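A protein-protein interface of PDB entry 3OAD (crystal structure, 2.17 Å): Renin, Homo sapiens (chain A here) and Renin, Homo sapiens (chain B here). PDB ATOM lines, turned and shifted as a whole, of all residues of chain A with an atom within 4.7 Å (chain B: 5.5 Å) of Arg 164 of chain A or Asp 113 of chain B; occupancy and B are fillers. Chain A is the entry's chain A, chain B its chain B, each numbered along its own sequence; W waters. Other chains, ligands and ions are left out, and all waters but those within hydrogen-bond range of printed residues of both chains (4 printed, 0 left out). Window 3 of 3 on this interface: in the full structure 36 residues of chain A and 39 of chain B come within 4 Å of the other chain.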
ATOM      1  N   ASN A  14      -9.846 -34.637  -5.942  1.00  0.00           N
ATOM      2  CA  ASN A  14      -9.634 -33.219  -5.773  1.00  0.00           C
ATOM      3  C   ASN A  14      -8.147 -32.913  -5.863  1.00  0.00           C
ATOM      4  O   ASN A  14      -7.395 -33.264  -4.954  1.00  0.00           O
ATOM      5  CB  ASN A  14     -10.136 -32.761  -4.401  1.00  0.00           C
ATOM      6  CG  ASN A  14      -9.846 -31.289  -4.146  1.00  0.00           C
ATOM      7  OD1 ASN A  14      -9.264 -30.611  -4.976  1.00  0.00           O
ATOM      8  ND2 ASN A  14     -10.223 -30.813  -3.002  1.00  0.00           N
ATOM      9  N   ASP A  17      -7.745 -28.176  -5.089  1.00  0.00           N
ATOM     10  CA  ASP A  17      -8.935 -27.344  -5.123  1.00  0.00           C
ATOM     11  C   ASP A  17      -9.159 -26.681  -6.503  1.00  0.00           C
ATOM     12  O   ASP A  17     -10.047 -25.812  -6.650  1.00  0.00           O
ATOM     13  CB  ASP A  17      -8.825 -26.227  -4.061  1.00  0.00           C
ATOM     14  CG  ASP A  17      -9.280 -26.640  -2.670  1.00  0.00           C
ATOM     15  OD1 ASP A  17      -9.828 -27.748  -2.446  1.00  0.00           O
ATOM     16  OD2 ASP A  17      -9.065 -25.806  -1.768  1.00  0.00           O
ATOM     17  N   TYR A 162     -18.313 -31.485  -4.441  1.00  0.00           N
ATOM     18  CA  TYR A 162     -16.863 -31.170  -4.471  1.00  0.00           C
ATOM     19  C   TYR A 162     -16.366 -30.936  -3.028  1.00  0.00           C
ATOM     20  O   TYR A 162     -16.749 -29.949  -2.397  1.00  0.00           O
ATOM     21  CB  TYR A 162     -16.595 -29.918  -5.321  1.00  0.00           C
ATOM     22  CG  TYR A 162     -16.575 -30.087  -6.828  1.00  0.00           C
ATOM     23  CD1 TYR A 162     -16.671 -31.347  -7.421  1.00  0.00           C
ATOM     24  CD2 TYR A 162     -16.428 -28.970  -7.672  1.00  0.00           C
ATOM     25  CE1 TYR A 162     -16.644 -31.503  -8.818  1.00  0.00           C
ATOM     26  CE2 TYR A 162     -16.412 -29.102  -9.071  1.00  0.00           C
ATOM     27  CZ  TYR A 162     -16.521 -30.386  -9.639  1.00  0.00           C
ATOM     28  OH  TYR A 162     -16.497 -30.572 -11.003  1.00  0.00           O
ATOM     29  N   ASN A 163     -15.555 -31.858  -2.499  1.00  0.00           N
ATOM     30  CA  ASN A 163     -14.881 -31.696  -1.191  1.00  0.00           C
ATOM     31  C   ASN A 163     -13.851 -30.548  -1.216  1.00  0.00           C
ATOM     32  O   ASN A 163     -13.550 -29.992  -2.274  1.00  0.00           O
ATOM     33  CB  ASN A 163     -14.175 -32.995  -0.818  1.00  0.00           C
ATOM     34  CG  ASN A 163     -13.986 -33.175   0.700  1.00  0.00           C
ATOM     35  OD1 ASN A 163     -14.240 -32.260   1.495  1.00  0.00           O
ATOM     36  ND2 ASN A 163     -13.517 -34.362   1.101  1.00  0.00           N
ATOM     37  N   ARG A 164     -13.319 -30.205  -0.051  1.00  0.00           N
ATOM     38  CA  ARG A 164     -12.198 -29.270   0.062  1.00  0.00           C
ATOM     39  C   ARG A 164     -10.939 -30.047   0.424  1.00  0.00           C
ATOM     40  O   ARG A 164     -11.020 -31.060   1.110  1.00  0.00           O
ATOM     41  CB  ARG A 164     -12.455 -28.237   1.159  1.00  0.00           C
ATOM     42  CG  ARG A 164     -13.753 -27.461   1.041  1.00  0.00           C
ATOM     43  CD  ARG A 164     -13.993 -26.629   2.307  1.00  0.00           C
ATOM     44  NE  ARG A 164     -15.417 -26.380   2.559  1.00  0.00           N
ATOM     45  CZ  ARG A 164     -16.190 -25.505   1.899  1.00  0.00           C
ATOM     46  NH1 ARG A 164     -15.704 -24.742   0.902  1.00  0.00           N
ATOM     47  NH2 ARG A 164     -17.478 -25.403   2.245  1.00  0.00           N
ATOM     48  N   ASP A 165      -9.778 -29.541   0.019  1.00  0.00           N
ATOM     49  CA  ASP A 165      -8.524 -30.268   0.193  1.00  0.00           C
ATOM     50  C   ASP A 165      -8.183 -30.518   1.668  1.00  0.00           C
ATOM     51  O   ASP A 165      -7.762 -29.626   2.409  1.00  0.00           O
ATOM     52  CB  ASP A 165      -7.370 -29.578  -0.558  1.00  0.00           C
ATOM     53  CG  ASP A 165      -6.456 -30.579  -1.286  1.00  0.00           C
ATOM     54  OD1 ASP A 165      -6.962 -31.563  -1.888  1.00  0.00           O
ATOM     55  OD2 ASP A 165      -5.220 -30.378  -1.266  1.00  0.00           O
ATOM     56  N   SER B   1     -10.250 -39.571   3.026  1.00  0.00           N
ATOM     57  CA  SER B   1     -10.521 -38.309   2.334  1.00  0.00           C
ATOM     58  C   SER B   1     -11.035 -38.542   0.910  1.00  0.00           C
ATOM     59  O   SER B   1     -10.310 -39.051   0.052  1.00  0.00           O
ATOM     60  CB  SER B   1      -9.268 -37.425   2.314  1.00  0.00           C
ATOM     61  OG  SER B   1      -9.559 -36.137   1.795  1.00  0.00           O
ATOM     62  N   GLY B   3     -12.380 -36.868  -2.524  1.00  0.00           N
ATOM     63  CA  GLY B   3     -12.159 -35.602  -3.238  1.00  0.00           C
ATOM     64  C   GLY B   3     -13.423 -34.930  -3.770  1.00  0.00           C
ATOM     65  O   GLY B   3     -13.428 -33.720  -4.035  1.00  0.00           O
ATOM     66  N   THR B 108     -23.786 -17.247  -0.011  1.00  0.00           N
ATOM     67  CA  THR B 108     -22.693 -16.524   0.647  1.00  0.00           C
ATOM     68  C   THR B 108     -21.450 -17.360   0.822  1.00  0.00           C
ATOM     69  O   THR B 108     -21.470 -18.439   1.434  1.00  0.00           O
ATOM     70  CB  THR B 108     -23.110 -15.977   2.047  1.00  0.00           C
ATOM     71  OG1 THR B 108     -24.197 -15.066   1.894  1.00  0.00           O
ATOM     72  CG2 THR B 108     -21.950 -15.223   2.726  1.00  0.00           C
ATOM     73  N   LEU B 109     -20.366 -16.839   0.280  1.00  0.00           N
ATOM     74  CA  LEU B 109     -19.049 -17.368   0.527  1.00  0.00           C
ATOM     75  C   LEU B 109     -18.314 -16.438   1.481  1.00  0.00           C
ATOM     76  O   LEU B 109     -18.383 -15.226   1.346  1.00  0.00           O
ATOM     77  CB  LEU B 109     -18.276 -17.499  -0.782  1.00  0.00           C
ATOM     78  CG  LEU B 109     -18.869 -18.236  -1.977  1.00  0.00           C
ATOM     79  CD1 LEU B 109     -17.776 -18.406  -2.995  1.00  0.00           C
ATOM     80  CD2 LEU B 109     -19.424 -19.596  -1.617  1.00  0.00           C
ATOM     81  N   THR B 110     -17.632 -17.019   2.458  1.00  0.00           N
ATOM     82  CA  THR B 110     -16.713 -16.282   3.315  1.00  0.00           C
ATOM     83  C   THR B 110     -15.293 -16.319   2.700  1.00  0.00           C
ATOM     84  O   THR B 110     -15.092 -16.877   1.604  1.00  0.00           O
ATOM     85  CB  THR B 110     -16.716 -16.840   4.733  1.00  0.00           C
ATOM     86  OG1 THR B 110     -16.189 -18.171   4.713  1.00  0.00           O
ATOM     87  CG2 THR B 110     -18.137 -16.903   5.267  1.00  0.00           C
ATOM     88  N   SER B 111     -14.321 -15.705   3.382  1.00  0.00           N
ATOM     89  CA  SER B 111     -12.931 -15.670   2.879  1.00  0.00           C
ATOM     90  C   SER B 111     -12.305 -17.052   2.863  1.00  0.00           C
ATOM     91  O   SER B 111     -11.529 -17.365   1.965  1.00  0.00           O
ATOM     92  CB  SER B 111     -12.047 -14.680   3.655  1.00  0.00           C
ATOM     93  OG  SER B 111     -12.232 -14.746   5.046  1.00  0.00           O
ATOM     94  N   ALA B 112     -12.676 -17.881   3.838  1.00  0.00           N
ATOM     95  CA  ALA B 112     -12.298 -19.296   3.834  1.00  0.00           C
ATOM     96  C   ALA B 112     -12.744 -20.027   2.570  1.00  0.00           C
ATOM     97  O   ALA B 112     -12.183 -21.075   2.227  1.00  0.00           O
ATOM     98  CB  ALA B 112     -12.848 -20.008   5.077  1.00  0.00           C
ATOM     99  N   ASP B 113     -13.765 -19.485   1.900  1.00  0.00           N
ATOM    100  CA  ASP B 113     -14.301 -20.111   0.706  1.00  0.00           C
ATOM    101  C   ASP B 113     -13.610 -19.664  -0.560  1.00  0.00           C
ATOM    102  O   ASP B 113     -13.622 -20.406  -1.549  1.00  0.00           O
ATOM    103  CB  ASP B 113     -15.829 -19.944   0.588  1.00  0.00           C
ATOM    104  CG  ASP B 113     -16.572 -20.473   1.798  1.00  0.00           C
ATOM    105  OD1 ASP B 113     -16.280 -21.628   2.219  1.00  0.00           O
ATOM    106  OD2 ASP B 113     -17.444 -19.737   2.349  1.00  0.00           O
ATOM    107  N   TYR B 114     -12.976 -18.486  -0.542  1.00  0.00           N
ATOM    108  CA  TYR B 114     -12.330 -17.962  -1.756  1.00  0.00           C
ATOM    109  C   TYR B 114     -10.863 -17.481  -1.653  1.00  0.00           C
ATOM    110  O   TYR B 114     -10.255 -17.170  -2.681  1.00  0.00           O
ATOM    111  CB  TYR B 114     -13.228 -16.913  -2.458  1.00  0.00           C
ATOM    112  CG  TYR B 114     -13.398 -15.623  -1.686  1.00  0.00           C
ATOM    113  CD1 TYR B 114     -12.427 -14.616  -1.759  1.00  0.00           C
ATOM    114  CD2 TYR B 114     -14.513 -15.415  -0.886  1.00  0.00           C
ATOM    115  CE1 TYR B 114     -12.558 -13.426  -1.042  1.00  0.00           C
ATOM    116  CE2 TYR B 114     -14.657 -14.241  -0.155  1.00  0.00           C
ATOM    117  CZ  TYR B 114     -13.665 -13.239  -0.243  1.00  0.00           C
ATOM    118  OH  TYR B 114     -13.793 -12.061   0.479  1.00  0.00           O
ATOM    119  N   VAL B 115     -10.275 -17.453  -0.460  1.00  0.00           N
ATOM    120  CA  VAL B 115      -8.847 -17.129  -0.348  1.00  0.00           C
ATOM    121  C   VAL B 115      -8.012 -18.397  -0.149  1.00  0.00           C
ATOM    122  O   VAL B 115      -8.317 -19.214   0.733  1.00  0.00           O
ATOM    123  CB  VAL B 115      -8.545 -16.063   0.801  1.00  0.00           C
ATOM    124  CG1 VAL B 115      -7.056 -15.810   0.945  1.00  0.00           C
ATOM    125  CG2 VAL B 115      -9.258 -14.728   0.541  1.00  0.00           C
ATOM    126  N   ALA B 129      -9.709 -17.266  -5.331  1.00  0.00           N
ATOM    127  CA  ALA B 129     -10.394 -18.254  -6.180  1.00  0.00           C
ATOM    128  C   ALA B 129     -11.466 -17.659  -7.097  1.00  0.00           C
ATOM    129  O   ALA B 129     -12.512 -18.286  -7.326  1.00  0.00           O
ATOM    130  CB  ALA B 129     -11.002 -19.364  -5.314  1.00  0.00           C
ATOM    131  N   THR B 148     -15.193 -23.146  -6.957  1.00  0.00           N
ATOM    132  CA  THR B 148     -15.205 -22.261  -5.806  1.00  0.00           C
ATOM    133  C   THR B 148     -16.595 -22.182  -5.205  1.00  0.00           C
ATOM    134  O   THR B 148     -16.747 -22.130  -3.974  1.00  0.00           O
ATOM    135  CB  THR B 148     -14.702 -20.853  -6.209  1.00  0.00           C
ATOM    136  OG1 THR B 148     -13.359 -20.974  -6.678  1.00  0.00           O
ATOM    137  CG2 THR B 148     -14.728 -19.868  -5.028  1.00  0.00           C
ATOM    138  N   ARG B 151     -17.980 -26.140  -4.361  1.00  0.00           N
ATOM    139  CA  ARG B 151     -17.478 -26.651  -3.062  1.00  0.00           C
ATOM    140  C   ARG B 151     -18.387 -26.258  -1.892  1.00  0.00           C
ATOM    141  O   ARG B 151     -18.576 -27.013  -0.949  1.00  0.00           O
ATOM    142  CB  ARG B 151     -16.091 -26.104  -2.737  1.00  0.00           C
ATOM    143  CG  ARG B 151     -14.899 -26.891  -3.238  1.00  0.00           C
ATOM    144  CD  ARG B 151     -13.628 -26.383  -2.554  1.00  0.00           C
ATOM    145  NE  ARG B 151     -13.267 -25.007  -2.964  1.00  0.00           N
ATOM    146  CZ  ARG B 151     -12.576 -24.705  -4.063  1.00  0.00           C
ATOM    147  NH1 ARG B 151     -12.164 -25.654  -4.893  1.00  0.00           N
ATOM    148  NH2 ARG B 151     -12.296 -23.446  -4.344  1.00  0.00           N
ATOM    149  N   LYS B 152     -18.931 -25.050  -1.928  1.00  0.00           N
ATOM    150  CA  LYS B 152     -19.802 -24.653  -0.850  1.00  0.00           C
ATOM    151  C   LYS B 152     -21.227 -25.169  -1.034  1.00  0.00           C
ATOM    152  O   LYS B 152     -21.897 -25.464  -0.047  1.00  0.00           O
ATOM    153  CB  LYS B 152     -19.809 -23.154  -0.661  1.00  0.00           C
ATOM    154  CG  LYS B 152     -20.525 -22.770   0.633  1.00  0.00           C
ATOM    155  CD  LYS B 152     -19.957 -21.511   1.257  1.00  0.00           C
ATOM    156  CE  LYS B 152     -20.669 -21.155   2.533  1.00  0.00           C
ATOM    157  NZ  LYS B 152     -19.831 -20.200   3.293  1.00  0.00           N
ATOM    158  N   ALA B 169     -23.275 -27.786   1.207  1.00  0.00           N
ATOM    159  CA  ALA B 169     -22.542 -29.045   1.237  1.00  0.00           C
ATOM    160  C   ALA B 169     -22.151 -29.418   2.664  1.00  0.00           C
ATOM    161  O   ALA B 169     -21.735 -28.548   3.436  1.00  0.00           O
ATOM    162  CB  ALA B 169     -21.337 -29.011   0.308  1.00  0.00           C
ATOM    163  N   HIS B 171     -19.472 -31.203   4.643  1.00  0.00           N
ATOM    164  CA  HIS B 171     -18.094 -31.684   4.583  1.00  0.00           C
ATOM    165  C   HIS B 171     -17.706 -32.441   5.868  1.00  0.00           C
ATOM    166  O   HIS B 171     -17.341 -33.628   5.809  1.00  0.00           O
ATOM    167  CB  HIS B 171     -17.119 -30.532   4.299  1.00  0.00           C
ATOM    168  CG  HIS B 171     -17.258 -29.944   2.928  1.00  0.00           C
ATOM    169  ND1 HIS B 171     -17.983 -28.798   2.681  1.00  0.00           N
ATOM    170  CD2 HIS B 171     -16.762 -30.340   1.730  1.00  0.00           C
ATOM    171  CE1 HIS B 171     -17.923 -28.512   1.391  1.00  0.00           C
ATOM    172  NE2 HIS B 171     -17.193 -29.433   0.789  1.00  0.00           N
HETATM  173  O   HOH W   1     -20.556 -26.309   2.495  1.00  0.00           O
HETATM  174  O   HOH W   2     -13.251 -23.897   2.766  1.00  0.00           O
HETATM  175  O   HOH W   3     -11.135 -23.490  -6.643  1.00  0.00           O
HETATM  176  O   HOH W   4     -14.873 -22.899  -1.753  1.00  0.00           O
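Printed residues of chain A that touch a printed residue of chain B: Asn 14, Asp 17, Tyr 162, Asn 163 and Arg 164.
Among the printed residues, Asp or Glu carboxylates within 4 Å of a Lys or Arg side-chain nitrogen of the other chain: Asp 17 of chain A with Arg 151 of chain B and Arg 164 of chain A with Asp 113 of chain B.
The backbone carbonyl oxygen (O) of Tyr 162 of chain A is in hydrogen-bond range of a ring nitrogen (NE2) of His 171 of chain B.
NH1 of Arg 164 of chain A is in salt-bridge range of OD1 of Asp 113 of chain B (3.4 Å).
ND1 of His 171 of chain B sits close to NH2 of Arg 164 of chain A, at 3.5 Å.
The backbone carbonyl oxygen of Gly 3 of chain B is in hydrogen-bond range of the backbone NH of Asn 163 of chain A (3.2 Å).
The side-chain carboxylate of Asp 17 of chain A lies within salt-bridge range of the guanidinium group of Arg 151 of chain B, 3.98 Å away.
N of Asp 165 of chain A lies close to ND2 of Asn 14 of chain A (3.3 Å).
The backbone NH (N) of Asp 17 of chain A lies within hydrogen-bond range of the side-chain amide oxygen (OD1) of Asn 14 of chain A (2.9 Å).
The backbone NH of Asp 165 of chain A sits at hydrogen-bond distance from the side-chain carboxylate of Asp 17 of chain A.
The side-chain carboxylate (OD2) of Asp 113 of chain B sits at hydrogen-bond distance from the backbone NH (N) of Thr 110 of chain B (2.7 Å).
OD2 of Asp 113 of chain B lies within salt-bridge range of NZ of Lys 152 of chain B.
O of Lys 152 of chain B sits at hydrogen-bond distance from N of Ala 169 of chain B.
Asn 14 of chain A touches Gly 3 of chain B.
Arg 151 of chain B touches Tyr 162 of chain A.
Asn 163 of chain A touches Arg 151 of chain B.
CD2 of His 171 of chain B touches OD1 of Asn 163 of chain A, 3.2 Å away.
Arg 164 of chain A touches Arg 151 of chain B.
Lys 152 of chain B touches Arg 164 of chain A (CA to NH2, 3.9 Å).
Water W3 lies within hydrogen-bond range of O of Asp 17 of chain A (2.6 Å), NH2 of Arg 151 of chain B (2.6 Å) and OG1 of Thr 148 of chain B (3.4 Å).
Water W1 lies within hydrogen-bond range of the backbone carbonyl oxygen (O) of Ala 169 of chain B (2.7 Å), the backbone carbonyl oxygen (O) of Lys 152 of chain B (3.0 Å) and the guanidinium group (NH2) of Arg 164 of chain A (3.2 Å).
Water W4 lies within hydrogen-bond range of the backbone carbonyl oxygen (O) of Asp 113 of chain B (2.8 Å), the guanidinium group (NE) of Arg 151 of chain B (2.9 Å), the backbone carbonyl oxygen (O) of Thr 148 of chain B (3.0 Å) and the guanidinium group (NH1) of Arg 164 of chain A (3.3 Å).
Water W2 lies within hydrogen-bond range of the backbone carbonyl oxygen of Ala 112 of chain B (3.1 Å) and the guanidinium group of Arg 164 of chain A (3.2 Å).
Of the printed residues of chain B, Asp 17 of chain A touches Arg 151 (2.8 Å).
Of the printed residues of chain B, Asn 163 of chain A touches Gly 3, Arg 151 and His 171.
Arg 164 of chain A touches four residues of chain B.
Asp 113 of chain B touches just one residue of chain A: Arg 164 (3.4 Å).
Val 115 of chain B touches none of the printed residues of chain A.
Of the printed residues of chain A, Lys 152 of chain B touches Arg 164.
The nearest printed residue of chain A that does not touch Asp 113 of chain B is Asp 17 of chain A (7.1 Å).
The nearest printed residue of chain A that does not touch His 171 of chain B is Asp 165 of chain A (7.2 Å).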
